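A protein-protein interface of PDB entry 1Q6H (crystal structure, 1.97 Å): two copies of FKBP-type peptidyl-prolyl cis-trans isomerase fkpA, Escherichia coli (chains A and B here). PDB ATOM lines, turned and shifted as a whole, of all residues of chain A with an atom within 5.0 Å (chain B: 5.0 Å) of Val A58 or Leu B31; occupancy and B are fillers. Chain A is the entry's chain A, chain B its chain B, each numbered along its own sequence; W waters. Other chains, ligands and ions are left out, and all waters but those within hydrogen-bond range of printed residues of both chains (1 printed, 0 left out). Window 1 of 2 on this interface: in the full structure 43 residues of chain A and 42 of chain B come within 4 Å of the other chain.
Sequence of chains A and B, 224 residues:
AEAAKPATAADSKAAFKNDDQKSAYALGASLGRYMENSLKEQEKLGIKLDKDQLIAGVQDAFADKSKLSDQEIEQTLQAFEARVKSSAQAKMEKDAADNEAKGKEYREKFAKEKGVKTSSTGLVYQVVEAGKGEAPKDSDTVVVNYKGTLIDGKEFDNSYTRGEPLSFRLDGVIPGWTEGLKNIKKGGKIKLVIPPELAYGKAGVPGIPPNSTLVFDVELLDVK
Water W1 bridges O of Ala A61 (2.6 Å) and NE of Arg B33 (3.2 Å).
Of the printed residues of chain B, Leu A54 touches Gly B28. Of the printed residues of chain B, Val A58 touches Gly B28 (3.3 Å), Ala B29 (3.8 Å), Leu B31 (3.96 Å), Gly B32 (3.9 Å) and Met B35 (3.8 Å). Of the printed residues of chain B, Ala A61 touches Ala B29. Of the printed residues of chain A, Gly B28 touches Leu A54, Gly A57 and Val A58. Of the printed residues of chain A, Ala B29 touches Gly A57, Val A58 and Ala A61. Of the printed residues of chain A, Leu B31 touches Val A58. Of the printed residues of chain A, Ile B55 touches Phe A62 (3.5 Å). The nearest printed residue of chain A that does not touch Leu B31 is Leu A31 (4.1 Å).
Of the 12 printed residues of chain A, 6 touch a printed residue of chain B. Printed residues of chain A that touch a printed residue of chain B: Leu A31, Leu A54, Gly A57, Val A58, Ala A61 and Phe A62. Hydrophobic or aromatic side chains of chain A within 4 Å of the printed part of chain B: Leu A31, Leu A54, Val A58, Ala A61 and Phe A62. Among the printed residues, no Asp or Glu carboxylate lies within 4 Å of a Lys or Arg side-chain nitrogen of the other chain.
N of Val A58 sits close to O of Gly B28 (3.5 Å).
Among the printed residues, pairs that only touch across the chains: Leu A31 with Met B35 (3.96 Å), Leu A54 with Gly B28 (3.4 Å), Gly A57 with Gly B28 (3.5 Å), Gly A57 with Ala B29 (3.3 Å), Val A58 with Ala B29 (3.8 Å), Val A58 with Leu B31 (3.96 Å), Val A58 with Gly B32 (3.9 Å), Val A58 with Met B35 (3.8 Å), Ala A61 with Ala B29 (3.3 Å), Phe A62 with Gly B32 (3.8 Å), Phe A62 with Met B35 (3.7 Å) and Phe A62 with Ile B55 (3.5 Å).
Leu A31 touches Met B35, but with the chains exchanged Met A35 does not touch Leu B31 (4.5 Å). Val A58 touches Leu B31, but with the chains exchanged Leu A31 does not touch Val B58 (4.5 Å). Val A58 touches Met B35, but with the chains exchanged Met A35 does not touch Val B58 (6.3 Å). Positions printed for both chains: 31, 35, 55 and 58.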
ATOM      1  N   LEU A  31      17.449 -28.907  12.579  1.00  0.00           N
ATOM      2  CA  LEU A  31      17.102 -27.708  13.340  1.00  0.00           C
ATOM      3  C   LEU A  31      18.281 -27.082  14.060  1.00  0.00           C
ATOM      4  O   LEU A  31      18.431 -25.872  14.080  1.00  0.00           O
ATOM      5  CB  LEU A  31      15.988 -28.016  14.324  1.00  0.00           C
ATOM      6  CG  LEU A  31      14.648 -28.310  13.640  1.00  0.00           C
ATOM      7  CD1 LEU A  31      13.642 -28.946  14.584  1.00  0.00           C
ATOM      8  CD2 LEU A  31      14.048 -27.055  13.036  1.00  0.00           C
ATOM      9  N   MET A  35      19.944 -23.334  13.466  1.00  0.00           N
ATOM     10  CA  MET A  35      20.208 -22.419  14.569  1.00  0.00           C
ATOM     11  C   MET A  35      21.681 -22.002  14.540  1.00  0.00           C
ATOM     12  O   MET A  35      22.006 -20.810  14.619  1.00  0.00           O
ATOM     13  CB  MET A  35      19.906 -23.119  15.903  1.00  0.00           C
ATOM     14  CG  MET A  35      19.515 -22.210  17.082  1.00  0.00           C
ATOM     15  SD  MET A  35      18.634 -20.576  16.559  1.00  0.00           S
ATOM     16  CE  MET A  35      17.003 -21.430  15.873  1.00  0.00           C
ATOM     17  N   LEU A  54      21.061 -20.621  24.999  1.00  0.00           N
ATOM     18  CA  LEU A  54      20.233 -20.997  23.857  1.00  0.00           C
ATOM     19  C   LEU A  54      19.752 -22.437  24.017  1.00  0.00           C
ATOM     20  O   LEU A  54      18.579 -22.702  23.856  1.00  0.00           O
ATOM     21  CB  LEU A  54      20.949 -20.772  22.530  1.00  0.00           C
ATOM     22  CG  LEU A  54      19.993 -20.804  21.335  1.00  0.00           C
ATOM     23  CD1 LEU A  54      20.442 -19.973  20.172  1.00  0.00           C
ATOM     24  CD2 LEU A  54      19.787 -22.235  20.903  1.00  0.00           C
ATOM     25  N   ILE A  55      20.639 -23.337  24.424  1.00  0.00           N
ATOM     26  CA  ILE A  55      20.245 -24.725  24.624  1.00  0.00           C
ATOM     27  C   ILE A  55      19.311 -24.873  25.848  1.00  0.00           C
ATOM     28  O   ILE A  55      18.405 -25.676  25.821  1.00  0.00           O
ATOM     29  CB  ILE A  55      21.485 -25.680  24.689  1.00  0.00           C
ATOM     30  CG1 ILE A  55      22.209 -25.699  23.352  1.00  0.00           C
ATOM     31  CG2 ILE A  55      21.067 -27.127  25.013  1.00  0.00           C
ATOM     32  CD1 ILE A  55      21.390 -26.202  22.138  1.00  0.00           C
ATOM     33  N   ALA A  56      19.511 -24.074  26.890  1.00  0.00           N
ATOM     34  CA  ALA A  56      18.627 -24.110  28.064  1.00  0.00           C
ATOM     35  C   ALA A  56      17.191 -23.677  27.660  1.00  0.00           C
ATOM     36  O   ALA A  56      16.217 -24.261  28.079  1.00  0.00           O
ATOM     37  CB  ALA A  56      19.162 -23.223  29.145  1.00  0.00           C
ATOM     38  N   GLY A  57      17.073 -22.662  26.819  1.00  0.00           N
ATOM     39  CA  GLY A  57      15.776 -22.281  26.310  1.00  0.00           C
ATOM     40  C   GLY A  57      15.109 -23.404  25.529  1.00  0.00           C
ATOM     41  O   GLY A  57      13.909 -23.671  25.682  1.00  0.00           O
ATOM     42  N   VAL A  58      15.866 -24.078  24.673  1.00  0.00           N
ATOM     43  CA  VAL A  58      15.281 -25.186  23.935  1.00  0.00           C
ATOM     44  C   VAL A  58      14.755 -26.231  24.906  1.00  0.00           C
ATOM     45  O   VAL A  58      13.595 -26.668  24.816  1.00  0.00           O
ATOM     46  CB  VAL A  58      16.289 -25.872  22.992  1.00  0.00           C
ATOM     47  CG1 VAL A  58      15.617 -27.050  22.286  1.00  0.00           C
ATOM     48  CG2 VAL A  58      16.879 -24.868  22.005  1.00  0.00           C
ATOM     49  N   GLN A  59      15.604 -26.633  25.835  1.00  0.00           N
ATOM     50  CA  GLN A  59      15.249 -27.685  26.785  1.00  0.00           C
ATOM     51  C   GLN A  59      14.030 -27.291  27.643  1.00  0.00           C
ATOM     52  O   GLN A  59      13.046 -28.065  27.777  1.00  0.00           O
ATOM     53  CB  GLN A  59      16.462 -28.013  27.671  1.00  0.00           C
ATOM     54  CG  GLN A  59      17.656 -28.652  26.901  1.00  0.00           C
ATOM     55  CD  GLN A  59      18.979 -28.633  27.663  1.00  0.00           C
ATOM     56  OE1 GLN A  59      19.890 -29.412  27.352  1.00  0.00           O
ATOM     57  NE2 GLN A  59      19.099 -27.747  28.638  1.00  0.00           N
ATOM     58  N   ASP A  60      14.099 -26.103  28.238  1.00  0.00           N
ATOM     59  CA  ASP A  60      13.036 -25.634  29.135  1.00  0.00           C
ATOM     60  C   ASP A  60      11.684 -25.551  28.375  1.00  0.00           C
ATOM     61  O   ASP A  60      10.657 -26.057  28.830  1.00  0.00           O
ATOM     62  CB  ASP A  60      13.395 -24.269  29.748  1.00  0.00           C
ATOM     63  CG  ASP A  60      14.563 -24.322  30.709  1.00  0.00           C
ATOM     64  OD1 ASP A  60      14.978 -25.426  31.111  1.00  0.00           O
ATOM     65  OD2 ASP A  60      15.134 -23.287  31.142  1.00  0.00           O
ATOM     66  N   ALA A  61      11.683 -24.945  27.201  1.00  0.00           N
ATOM     67  CA  ALA A  61      10.444 -24.858  26.427  1.00  0.00           C
ATOM     68  C   ALA A  61       9.931 -26.241  25.992  1.00  0.00           C
ATOM     69  O   ALA A  61       8.718 -26.531  26.027  1.00  0.00           O
ATOM     70  CB  ALA A  61      10.635 -23.973  25.238  1.00  0.00           C
ATOM     71  N   PHE A  62      10.841 -27.117  25.617  1.00  0.00           N
ATOM     72  CA  PHE A  62      10.434 -28.433  25.138  1.00  0.00           C
ATOM     73  C   PHE A  62       9.751 -29.188  26.293  1.00  0.00           C
ATOM     74  O   PHE A  62       8.920 -30.076  26.090  1.00  0.00           O
ATOM     75  CB  PHE A  62      11.660 -29.173  24.628  1.00  0.00           C
ATOM     76  CG  PHE A  62      11.353 -30.332  23.753  1.00  0.00           C
ATOM     77  CD1 PHE A  62      10.592 -30.177  22.604  1.00  0.00           C
ATOM     78  CD2 PHE A  62      11.829 -31.586  24.072  1.00  0.00           C
ATOM     79  CE1 PHE A  62      10.313 -31.257  21.792  1.00  0.00           C
ATOM     80  CE2 PHE A  62      11.553 -32.685  23.249  1.00  0.00           C
ATOM     81  CZ  PHE A  62      10.793 -32.511  22.113  1.00  0.00           C
ATOM     82  N   ALA A  63      10.087 -28.804  27.513  1.00  0.00           N
ATOM     83  CA  ALA A  63       9.524 -29.435  28.680  1.00  0.00           C
ATOM     84  C   ALA A  63       8.381 -28.606  29.276  1.00  0.00           C
ATOM     85  O   ALA A  63       7.879 -28.919  30.360  1.00  0.00           O
ATOM     86  CB  ALA A  63      10.625 -29.667  29.692  1.00  0.00           C
ATOM     87  N   LEU B  27      15.410 -17.196  21.868  1.00  0.00           N
ATOM     88  CA  LEU B  27      15.564 -17.837  20.591  1.00  0.00           C
ATOM     89  C   LEU B  27      15.454 -19.342  20.759  1.00  0.00           C
ATOM     90  O   LEU B  27      14.737 -19.985  20.011  1.00  0.00           O
ATOM     91  CB  LEU B  27      16.917 -17.472  19.952  1.00  0.00           C
ATOM     92  CG  LEU B  27      16.862 -16.420  18.872  1.00  0.00           C
ATOM     93  CD1 LEU B  27      18.291 -16.156  18.293  1.00  0.00           C
ATOM     94  CD2 LEU B  27      15.920 -16.844  17.770  1.00  0.00           C
ATOM     95  N   GLY B  28      16.128 -19.876  21.770  1.00  0.00           N
ATOM     96  CA  GLY B  28      16.045 -21.289  22.086  1.00  0.00           C
ATOM     97  C   GLY B  28      14.640 -21.774  22.437  1.00  0.00           C
ATOM     98  O   GLY B  28      14.173 -22.778  21.946  1.00  0.00           O
ATOM     99  N   ALA B  29      13.979 -21.054  23.330  1.00  0.00           N
ATOM    100  CA  ALA B  29      12.620 -21.384  23.745  1.00  0.00           C
ATOM    101  C   ALA B  29      11.708 -21.400  22.527  1.00  0.00           C
ATOM    102  O   ALA B  29      10.814 -22.225  22.406  1.00  0.00           O
ATOM    103  CB  ALA B  29      12.131 -20.352  24.792  1.00  0.00           C
ATOM    104  N   SER B  30      11.948 -20.493  21.603  1.00  0.00           N
ATOM    105  CA  SER B  30      11.148 -20.448  20.409  1.00  0.00           C
ATOM    106  C   SER B  30      11.340 -21.702  19.574  1.00  0.00           C
ATOM    107  O   SER B  30      10.388 -22.211  18.952  1.00  0.00           O
ATOM    108  CB  SER B  30      11.460 -19.209  19.601  1.00  0.00           C
ATOM    109  OG  SER B  30      10.673 -19.207  18.435  1.00  0.00           O
ATOM    110  N   LEU B  31      12.558 -22.223  19.575  1.00  0.00           N
ATOM    111  CA  LEU B  31      12.813 -23.438  18.838  1.00  0.00           C
ATOM    112  C   LEU B  31      12.144 -24.576  19.572  1.00  0.00           C
ATOM    113  O   LEU B  31      11.511 -25.434  18.961  1.00  0.00           O
ATOM    114  CB  LEU B  31      14.307 -23.711  18.729  1.00  0.00           C
ATOM    115  CG  LEU B  31      14.628 -25.080  18.124  1.00  0.00           C
ATOM    116  CD1 LEU B  31      14.094 -25.176  16.708  1.00  0.00           C
ATOM    117  CD2 LEU B  31      16.122 -25.267  18.138  1.00  0.00           C
ATOM    118  N   GLY B  32      12.284 -24.594  20.883  1.00  0.00           N
ATOM    119  CA  GLY B  32      11.645 -25.654  21.655  1.00  0.00           C
ATOM    120  C   GLY B  32      10.124 -25.703  21.444  1.00  0.00           C
ATOM    121  O   GLY B  32       9.502 -26.769  21.293  1.00  0.00           O
ATOM    122  N   ARG B  33       9.526 -24.530  21.417  1.00  0.00           N
ATOM    123  CA  ARG B  33       8.107 -24.410  21.185  1.00  0.00           C
ATOM    124  C   ARG B  33       7.716 -24.955  19.810  1.00  0.00           C
ATOM    125  O   ARG B  33       6.708 -25.662  19.653  1.00  0.00           O
ATOM    126  CB  ARG B  33       7.718 -22.948  21.301  1.00  0.00           C
ATOM    127  CG  ARG B  33       6.353 -22.640  20.779  1.00  0.00           C
ATOM    128  CD  ARG B  33       5.268 -23.513  21.348  1.00  0.00           C
ATOM    129  NE  ARG B  33       5.231 -23.463  22.808  1.00  0.00           N
ATOM    130  CZ  ARG B  33       4.782 -22.427  23.522  1.00  0.00           C
ATOM    131  NH1 ARG B  33       4.327 -21.321  22.933  1.00  0.00           N
ATOM    132  NH2 ARG B  33       4.795 -22.495  24.840  1.00  0.00           N
ATOM    133  N   TYR B  34       8.528 -24.627  18.820  1.00  0.00           N
ATOM    134  CA  TYR B  34       8.310 -25.076  17.458  1.00  0.00           C
ATOM    135  C   TYR B  34       8.325 -26.609  17.357  1.00  0.00           C
ATOM    136  O   TYR B  34       7.483 -27.213  16.707  1.00  0.00           O
ATOM    137  CB  TYR B  34       9.349 -24.451  16.522  1.00  0.00           C
ATOM    138  CG  TYR B  34       9.289 -24.990  15.122  1.00  0.00           C
ATOM    139  CD1 TYR B  34       8.440 -24.450  14.176  1.00  0.00           C
ATOM    140  CD2 TYR B  34      10.072 -26.074  14.757  1.00  0.00           C
ATOM    141  CE1 TYR B  34       8.383 -24.979  12.898  1.00  0.00           C
ATOM    142  CE2 TYR B  34      10.037 -26.590  13.515  1.00  0.00           C
ATOM    143  CZ  TYR B  34       9.187 -26.059  12.585  1.00  0.00           C
ATOM    144  OH  TYR B  34       9.183 -26.606  11.337  1.00  0.00           O
ATOM    145  N   MET B  35       9.274 -27.225  18.032  1.00  0.00           N
ATOM    146  CA  MET B  35       9.370 -28.656  18.027  1.00  0.00           C
ATOM    147  C   MET B  35       8.134 -29.304  18.677  1.00  0.00           C
ATOM    148  O   MET B  35       7.576 -30.259  18.144  1.00  0.00           O
ATOM    149  CB  MET B  35      10.654 -29.086  18.783  1.00  0.00           C
ATOM    150  CG  MET B  35      11.993 -28.582  18.162  1.00  0.00           C
ATOM    151  SD  MET B  35      13.530 -28.413  19.422  1.00  0.00           S
ATOM    152  CE  MET B  35      13.523 -30.218  20.144  1.00  0.00           C
ATOM    153  N   ILE B  55      15.770 -34.097  20.764  1.00  0.00           N
ATOM    154  CA  ILE B  55      16.578 -33.150  21.516  1.00  0.00           C
ATOM    155  C   ILE B  55      18.079 -33.404  21.310  1.00  0.00           C
ATOM    156  O   ILE B  55      18.847 -32.457  21.164  1.00  0.00           O
ATOM    157  CB  ILE B  55      16.187 -33.202  23.012  1.00  0.00           C
ATOM    158  CG1 ILE B  55      15.272 -32.023  23.344  1.00  0.00           C
ATOM    159  CG2 ILE B  55      17.397 -33.146  23.921  1.00  0.00           C
ATOM    160  CD1 ILE B  55      16.019 -30.770  23.841  1.00  0.00           C
ATOM    161  N   VAL B  58      19.396 -31.925  18.105  1.00  0.00           N
ATOM    162  CA  VAL B  58      19.545 -30.485  18.266  1.00  0.00           C
ATOM    163  C   VAL B  58      20.845 -30.189  19.022  1.00  0.00           C
ATOM    164  O   VAL B  58      21.680 -29.433  18.542  1.00  0.00           O
ATOM    165  CB  VAL B  58      18.373 -29.851  19.001  1.00  0.00           C
ATOM    166  CG1 VAL B  58      18.692 -28.350  19.290  1.00  0.00           C
ATOM    167  CG2 VAL B  58      17.066 -30.011  18.202  1.00  0.00           C
HETATM  168  O   HOH W   1       6.651 -25.333  24.926  1.00  0.00           O
